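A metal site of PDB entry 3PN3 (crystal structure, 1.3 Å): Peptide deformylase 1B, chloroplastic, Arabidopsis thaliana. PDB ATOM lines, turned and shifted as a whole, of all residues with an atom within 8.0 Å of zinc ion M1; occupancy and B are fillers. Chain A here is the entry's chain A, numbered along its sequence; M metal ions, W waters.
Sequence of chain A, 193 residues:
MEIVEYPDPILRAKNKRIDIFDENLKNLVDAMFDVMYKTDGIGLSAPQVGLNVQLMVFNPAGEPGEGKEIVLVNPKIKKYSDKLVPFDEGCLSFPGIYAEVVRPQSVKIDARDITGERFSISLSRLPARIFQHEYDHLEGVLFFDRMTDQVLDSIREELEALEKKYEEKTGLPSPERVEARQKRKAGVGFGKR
OE2 of Glu 89 lies within hydrogen-bond range of ND1 of His 133, 2.7 Å away. NE2 of His 137 sits close to NE2 of Gln 48 (3.4 Å). N of Ser 93 lies close to SG of Cys 91. NE2 of Gln 48 sits at hydrogen-bond distance from OG of Ser 93 (2.9 Å). The side-chain hydroxyl (OG) of Ser 45 sits close to the side-chain amide oxygen (OE1) of Gln 48 (3.4 Å). The backbone carbonyl oxygen (O) of Gln 48 is in hydrogen-bond range of the backbone NH (N) of Val 4 (2.8 Å).
Zinc ion M1 is bound by water W1 (2.0 Å), a ring nitrogen (NE2) of His 133 (2.0 Å), a ring nitrogen (NE2) of His 137 (2.1 Å) and the side-chain sulfur of Cys 91 (2.3 Å). Zinc ion M1 has four donor atoms within binding distance.
Gln 48 touches zinc ion M1. Of the 22 residues printed, 4 come within 4 Å of zinc ion M1. Along chain A the residues within 4 Å of zinc ion M1 span positions 48 to 137. The nearest printed residue that does not touch zinc ion M1 is Glu 134 (4.1 Å).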
ATOM      1  N   ILE A   3      27.582   0.920  14.564  1.00  0.00           N
ATOM      2  CA  ILE A   3      27.431   2.087  15.429  1.00  0.00           C
ATOM      3  C   ILE A   3      26.965   1.573  16.778  1.00  0.00           C
ATOM      4  O   ILE A   3      25.932   0.901  16.887  1.00  0.00           O
ATOM      5  CB  ILE A   3      26.455   3.128  14.839  1.00  0.00           C
ATOM      6  CG1 ILE A   3      27.050   3.791  13.574  1.00  0.00           C
ATOM      7  CG2 ILE A   3      26.062   4.173  15.902  1.00  0.00           C
ATOM      8  CD1 ILE A   3      28.273   4.680  13.814  1.00  0.00           C
ATOM      9  N   VAL A   4      27.749   1.880  17.800  1.00  0.00           N
ATOM     10  CA  VAL A   4      27.451   1.507  19.182  1.00  0.00           C
ATOM     11  C   VAL A   4      26.284   2.360  19.687  1.00  0.00           C
ATOM     12  O   VAL A   4      26.292   3.576  19.515  1.00  0.00           O
ATOM     13  CB  VAL A   4      28.709   1.721  20.066  1.00  0.00           C
ATOM     14  CG1 VAL A   4      28.390   1.510  21.534  1.00  0.00           C
ATOM     15  CG2 VAL A   4      29.819   0.776  19.630  1.00  0.00           C
ATOM     16  N   LEU A  11      30.323   4.034  25.169  1.00  0.00           N
ATOM     17  CA  LEU A  11      30.023   5.448  24.949  1.00  0.00           C
ATOM     18  C   LEU A  11      30.318   6.352  26.142  1.00  0.00           C
ATOM     19  O   LEU A  11      30.245   7.572  26.025  1.00  0.00           O
ATOM     20  CB  LEU A  11      28.570   5.627  24.510  1.00  0.00           C
ATOM     21  CG  LEU A  11      28.170   4.914  23.220  1.00  0.00           C
ATOM     22  CD1 LEU A  11      26.681   5.009  23.011  1.00  0.00           C
ATOM     23  CD2 LEU A  11      28.923   5.450  21.994  1.00  0.00           C
ATOM     24  N   GLY A  43      30.542  14.321  10.956  1.00  0.00           N
ATOM     25  CA  GLY A  43      31.642  13.899  11.810  1.00  0.00           C
ATOM     26  C   GLY A  43      31.352  12.566  12.458  1.00  0.00           C
ATOM     27  O   GLY A  43      30.187  12.209  12.618  1.00  0.00           O
ATOM     28  N   LEU A  44      32.399  11.841  12.815  1.00  0.00           N
ATOM     29  CA  LEU A  44      32.258  10.557  13.494  1.00  0.00           C
ATOM     30  C   LEU A  44      33.411  10.361  14.461  1.00  0.00           C
ATOM     31  O   LEU A  44      34.575  10.523  14.097  1.00  0.00           O
ATOM     32  CB  LEU A  44      32.204   9.393  12.495  1.00  0.00           C
ATOM     33  CG  LEU A  44      32.145   7.976  13.081  1.00  0.00           C
ATOM     34  CD1 LEU A  44      30.896   7.723  13.917  1.00  0.00           C
ATOM     35  CD2 LEU A  44      32.232   6.949  11.966  1.00  0.00           C
ATOM     36  N   SER A  45      33.056   9.997  15.692  1.00  0.00           N
ATOM     37  CA  SER A  45      34.015   9.770  16.768  1.00  0.00           C
ATOM     38  C   SER A  45      34.270   8.270  16.949  1.00  0.00           C
ATOM     39  O   SER A  45      33.354   7.463  16.798  1.00  0.00           O
ATOM     40  CB  SER A  45      33.472  10.352  18.061  1.00  0.00           C
ATOM     41  OG  SER A  45      32.203   9.790  18.361  1.00  0.00           O
ATOM     42  N   GLN A  48      31.988   5.701  18.914  1.00  0.00           N
ATOM     43  CA  GLN A  48      30.755   5.281  18.250  1.00  0.00           C
ATOM     44  C   GLN A  48      30.910   4.087  17.321  1.00  0.00           C
ATOM     45  O   GLN A  48      29.913   3.446  16.985  1.00  0.00           O
ATOM     46  CB  GLN A  48      30.124   6.448  17.504  1.00  0.00           C
ATOM     47  CG  GLN A  48      29.426   7.414  18.414  1.00  0.00           C
ATOM     48  CD  GLN A  48      28.590   8.376  17.636  1.00  0.00           C
ATOM     49  OE1 GLN A  48      29.119   9.301  17.018  1.00  0.00           O
ATOM     50  NE2 GLN A  48      27.284   8.162  17.642  1.00  0.00           N
ATOM     51  N   GLU A  89      18.797  18.310  17.640  1.00  0.00           N
ATOM     52  CA  GLU A  89      19.966  17.472  17.485  1.00  0.00           C
ATOM     53  C   GLU A  89      19.597  15.996  17.495  1.00  0.00           C
ATOM     54  O   GLU A  89      18.672  15.579  18.195  1.00  0.00           O
ATOM     55  CB  GLU A  89      20.925  17.778  18.636  1.00  0.00           C
ATOM     56  CG  GLU A  89      22.387  17.506  18.359  1.00  0.00           C
ATOM     57  CD  GLU A  89      23.269  18.013  19.488  1.00  0.00           C
ATOM     58  OE1 GLU A  89      23.393  19.246  19.675  1.00  0.00           O
ATOM     59  OE2 GLU A  89      23.838  17.163  20.192  1.00  0.00           O
ATOM     60  N   GLY A  90      20.333  15.210  16.714  1.00  0.00           N
ATOM     61  CA  GLY A  90      20.204  13.761  16.725  1.00  0.00           C
ATOM     62  C   GLY A  90      21.522  13.108  17.076  1.00  0.00           C
ATOM     63  O   GLY A  90      22.529  13.783  17.305  1.00  0.00           O
ATOM     64  N   CYS A  91      21.513  11.776  17.117  1.00  0.00           N
ATOM     65  CA  CYS A  91      22.693  10.990  17.455  1.00  0.00           C
ATOM     66  C   CYS A  91      22.503   9.562  16.976  1.00  0.00           C
ATOM     67  O   CYS A  91      21.533   8.918  17.336  1.00  0.00           O
ATOM     68  CB  CYS A  91      22.923  10.980  18.975  1.00  0.00           C
ATOM     69  SG  CYS A  91      24.378  10.015  19.502  1.00  0.00           S
ATOM     70  N   LEU A  92      23.440   9.056  16.169  1.00  0.00           N
ATOM     71  CA  LEU A  92      23.342   7.691  15.659  1.00  0.00           C
ATOM     72  C   LEU A  92      23.289   6.629  16.758  1.00  0.00           C
ATOM     73  O   LEU A  92      22.808   5.525  16.536  1.00  0.00           O
ATOM     74  CB  LEU A  92      24.479   7.393  14.681  1.00  0.00           C
ATOM     75  CG  LEU A  92      24.497   8.148  13.350  1.00  0.00           C
ATOM     76  CD1 LEU A  92      25.691   7.699  12.533  1.00  0.00           C
ATOM     77  CD2 LEU A  92      23.204   7.951  12.574  1.00  0.00           C
ATOM     78  N   SER A  93      23.814   6.965  17.942  1.00  0.00           N
ATOM     79  CA  SER A  93      23.772   6.050  19.074  1.00  0.00           C
ATOM     80  C   SER A  93      22.391   5.989  19.752  1.00  0.00           C
ATOM     81  O   SER A  93      22.170   5.153  20.634  1.00  0.00           O
ATOM     82  CB  SER A  93      24.849   6.421  20.094  1.00  0.00           C
ATOM     83  OG  SER A  93      26.137   6.264  19.517  1.00  0.00           O
ATOM     84  N   PHE A  94      21.488   6.872  19.340  1.00  0.00           N
ATOM     85  CA  PHE A  94      20.117   6.918  19.842  1.00  0.00           C
ATOM     86  C   PHE A  94      19.192   6.959  18.626  1.00  0.00           C
ATOM     87  O   PHE A  94      18.645   8.006  18.297  1.00  0.00           O
ATOM     88  CB  PHE A  94      19.889   8.193  20.671  1.00  0.00           C
ATOM     89  CG  PHE A  94      20.746   8.305  21.911  1.00  0.00           C
ATOM     90  CD1 PHE A  94      22.079   8.695  21.829  1.00  0.00           C
ATOM     91  CD2 PHE A  94      20.180   8.100  23.175  1.00  0.00           C
ATOM     92  CE1 PHE A  94      22.854   8.837  22.983  1.00  0.00           C
ATOM     93  CE2 PHE A  94      20.946   8.251  24.323  1.00  0.00           C
ATOM     94  CZ  PHE A  94      22.281   8.614  24.230  1.00  0.00           C
ATOM     95  N   ARG A 103      23.772  24.906  22.408  1.00  0.00           N
ATOM     96  CA  ARG A 103      25.238  24.873  22.416  1.00  0.00           C
ATOM     97  C   ARG A 103      25.804  26.192  21.902  1.00  0.00           C
ATOM     98  O   ARG A 103      25.117  26.918  21.188  1.00  0.00           O
ATOM     99  CB  ARG A 103      25.777  23.779  21.499  1.00  0.00           C
ATOM    100  CG  ARG A 103      25.527  22.343  21.930  1.00  0.00           C
ATOM    101  CD  ARG A 103      26.226  21.406  20.966  1.00  0.00           C
ATOM    102  NE  ARG A 103      25.753  20.029  21.113  1.00  0.00           N
ATOM    103  CZ  ARG A 103      26.294  19.124  21.917  1.00  0.00           C
ATOM    104  NH1 ARG A 103      27.353  19.418  22.663  1.00  0.00           N
ATOM    105  NH2 ARG A 103      25.768  17.907  21.959  1.00  0.00           N
ATOM    106  N   ILE A 130      28.009  19.976  14.914  1.00  0.00           N
ATOM    107  CA  ILE A 130      28.371  18.569  14.794  1.00  0.00           C
ATOM    108  C   ILE A 130      29.680  18.294  15.516  1.00  0.00           C
ATOM    109  O   ILE A 130      29.822  17.295  16.227  1.00  0.00           O
ATOM    110  CB  ILE A 130      28.443  18.121  13.320  1.00  0.00           C
ATOM    111  CG1 ILE A 130      27.088  18.295  12.618  1.00  0.00           C
ATOM    112  CG2 ILE A 130      28.953  16.670  13.218  1.00  0.00           C
ATOM    113  CD1 ILE A 130      25.917  17.530  13.237  1.00  0.00           C
ATOM    114  N   HIS A 133      29.083  18.028  19.230  1.00  0.00           N
ATOM    115  CA  HIS A 133      28.411  16.774  19.502  1.00  0.00           C
ATOM    116  C   HIS A 133      29.397  15.589  19.508  1.00  0.00           C
ATOM    117  O   HIS A 133      29.393  14.765  20.433  1.00  0.00           O
ATOM    118  CB  HIS A 133      27.299  16.557  18.491  1.00  0.00           C
ATOM    119  CG  HIS A 133      26.593  15.249  18.662  1.00  0.00           C
ATOM    120  ND1 HIS A 133      25.379  15.140  19.311  1.00  0.00           N
ATOM    121  CD2 HIS A 133      26.947  13.997  18.300  1.00  0.00           C
ATOM    122  CE1 HIS A 133      25.013  13.864  19.332  1.00  0.00           C
ATOM    123  NE2 HIS A 133      25.951  13.151  18.726  1.00  0.00           N
ATOM    124  N   GLU A 134      30.246  15.524  18.493  1.00  0.00           N
ATOM    125  CA  GLU A 134      31.241  14.458  18.391  1.00  0.00           C
ATOM    126  C   GLU A 134      32.363  14.578  19.418  1.00  0.00           C
ATOM    127  O   GLU A 134      32.870  13.569  19.896  1.00  0.00           O
ATOM    128  CB  GLU A 134      31.797  14.383  16.967  1.00  0.00           C
ATOM    129  CG  GLU A 134      30.744  14.039  15.922  1.00  0.00           C
ATOM    130  CD  GLU A 134      30.136  12.655  16.147  1.00  0.00           C
ATOM    131  OE1 GLU A 134      30.883  11.728  16.529  1.00  0.00           O
ATOM    132  OE2 GLU A 134      28.913  12.502  15.951  1.00  0.00           O
ATOM    133  N   ASP A 136      31.962  15.829  22.426  1.00  0.00           N
ATOM    134  CA  ASP A 136      31.343  15.276  23.618  1.00  0.00           C
ATOM    135  C   ASP A 136      31.501  13.752  23.651  1.00  0.00           C
ATOM    136  O   ASP A 136      31.852  13.194  24.687  1.00  0.00           O
ATOM    137  CB  ASP A 136      29.861  15.647  23.698  1.00  0.00           C
ATOM    138  CG  ASP A 136      29.615  17.032  24.280  1.00  0.00           C
ATOM    139  OD1 ASP A 136      28.432  17.406  24.356  1.00  0.00           O
ATOM    140  OD2 ASP A 136      30.570  17.737  24.678  1.00  0.00           O
ATOM    141  N   HIS A 137      31.277  13.069  22.523  1.00  0.00           N
ATOM    142  CA  HIS A 137      31.471  11.615  22.481  1.00  0.00           C
ATOM    143  C   HIS A 137      32.888  11.231  22.933  1.00  0.00           C
ATOM    144  O   HIS A 137      33.057  10.225  23.627  1.00  0.00           O
ATOM    145  CB  HIS A 137      31.254  11.056  21.077  1.00  0.00           C
ATOM    146  CG  HIS A 137      29.823  10.785  20.742  1.00  0.00           C
ATOM    147  ND1 HIS A 137      29.050   9.860  21.423  1.00  0.00           N
ATOM    148  CD2 HIS A 137      29.025  11.272  19.746  1.00  0.00           C
ATOM    149  CE1 HIS A 137      27.843   9.823  20.892  1.00  0.00           C
ATOM    150  NE2 HIS A 137      27.803  10.660  19.870  1.00  0.00           N
ATOM    151  N   VAL A 141      30.528  12.005  26.899  1.00  0.00           N
ATOM    152  CA  VAL A 141      29.348  12.829  27.147  1.00  0.00           C
ATOM    153  C   VAL A 141      28.359  12.618  26.004  1.00  0.00           C
ATOM    154  O   VAL A 141      28.729  12.645  24.836  1.00  0.00           O
ATOM    155  CB  VAL A 141      29.737  14.325  27.304  1.00  0.00           C
ATOM    156  CG1 VAL A 141      28.510  15.222  27.337  1.00  0.00           C
ATOM    157  CG2 VAL A 141      30.580  14.530  28.559  1.00  0.00           C
ATOM    158  N   LEU A 142      27.094  12.382  26.363  1.00  0.00           N
ATOM    159  CA  LEU A 142      26.050  12.080  25.386  1.00  0.00           C
ATOM    160  C   LEU A 142      25.023  13.212  25.355  1.00  0.00           C
ATOM    161  O   LEU A 142      24.887  13.948  26.333  1.00  0.00           O
ATOM    162  CB  LEU A 142      25.397  10.739  25.710  1.00  0.00           C
ATOM    163  CG  LEU A 142      26.377   9.560  25.718  1.00  0.00           C
ATOM    164  CD1 LEU A 142      25.659   8.246  26.060  1.00  0.00           C
ATOM    165  CD2 LEU A 142      27.116   9.433  24.380  1.00  0.00           C
ATOM    166  N   PHE A 143      24.312  13.345  24.245  1.00  0.00           N
ATOM    167  CA  PHE A 143      23.582  14.585  23.980  1.00  0.00           C
ATOM    168  C   PHE A 143      22.443  14.900  24.955  1.00  0.00           C
ATOM    169  O   PHE A 143      22.121  16.062  25.181  1.00  0.00           O
ATOM    170  CB  PHE A 143      23.198  14.753  22.497  1.00  0.00           C
ATOM    171  CG  PHE A 143      22.014  13.920  22.025  1.00  0.00           C
ATOM    172  CD1 PHE A 143      21.158  14.451  21.063  1.00  0.00           C
ATOM    173  CD2 PHE A 143      21.768  12.637  22.492  1.00  0.00           C
ATOM    174  CE1 PHE A 143      20.076  13.734  20.579  1.00  0.00           C
ATOM    175  CE2 PHE A 143      20.673  11.902  22.014  1.00  0.00           C
ATOM    176  CZ  PHE A 143      19.822  12.457  21.050  1.00  0.00           C
HETATM  177 ZN    ZN M   1      26.167  11.143  18.664  1.00  0.00          ZN
HETATM  178 ZN    ZN M   2      28.291  10.671  15.878  1.00  0.00          ZN
HETATM  179  O   HOH W   1      26.592  10.740  16.796  1.00  0.00           O
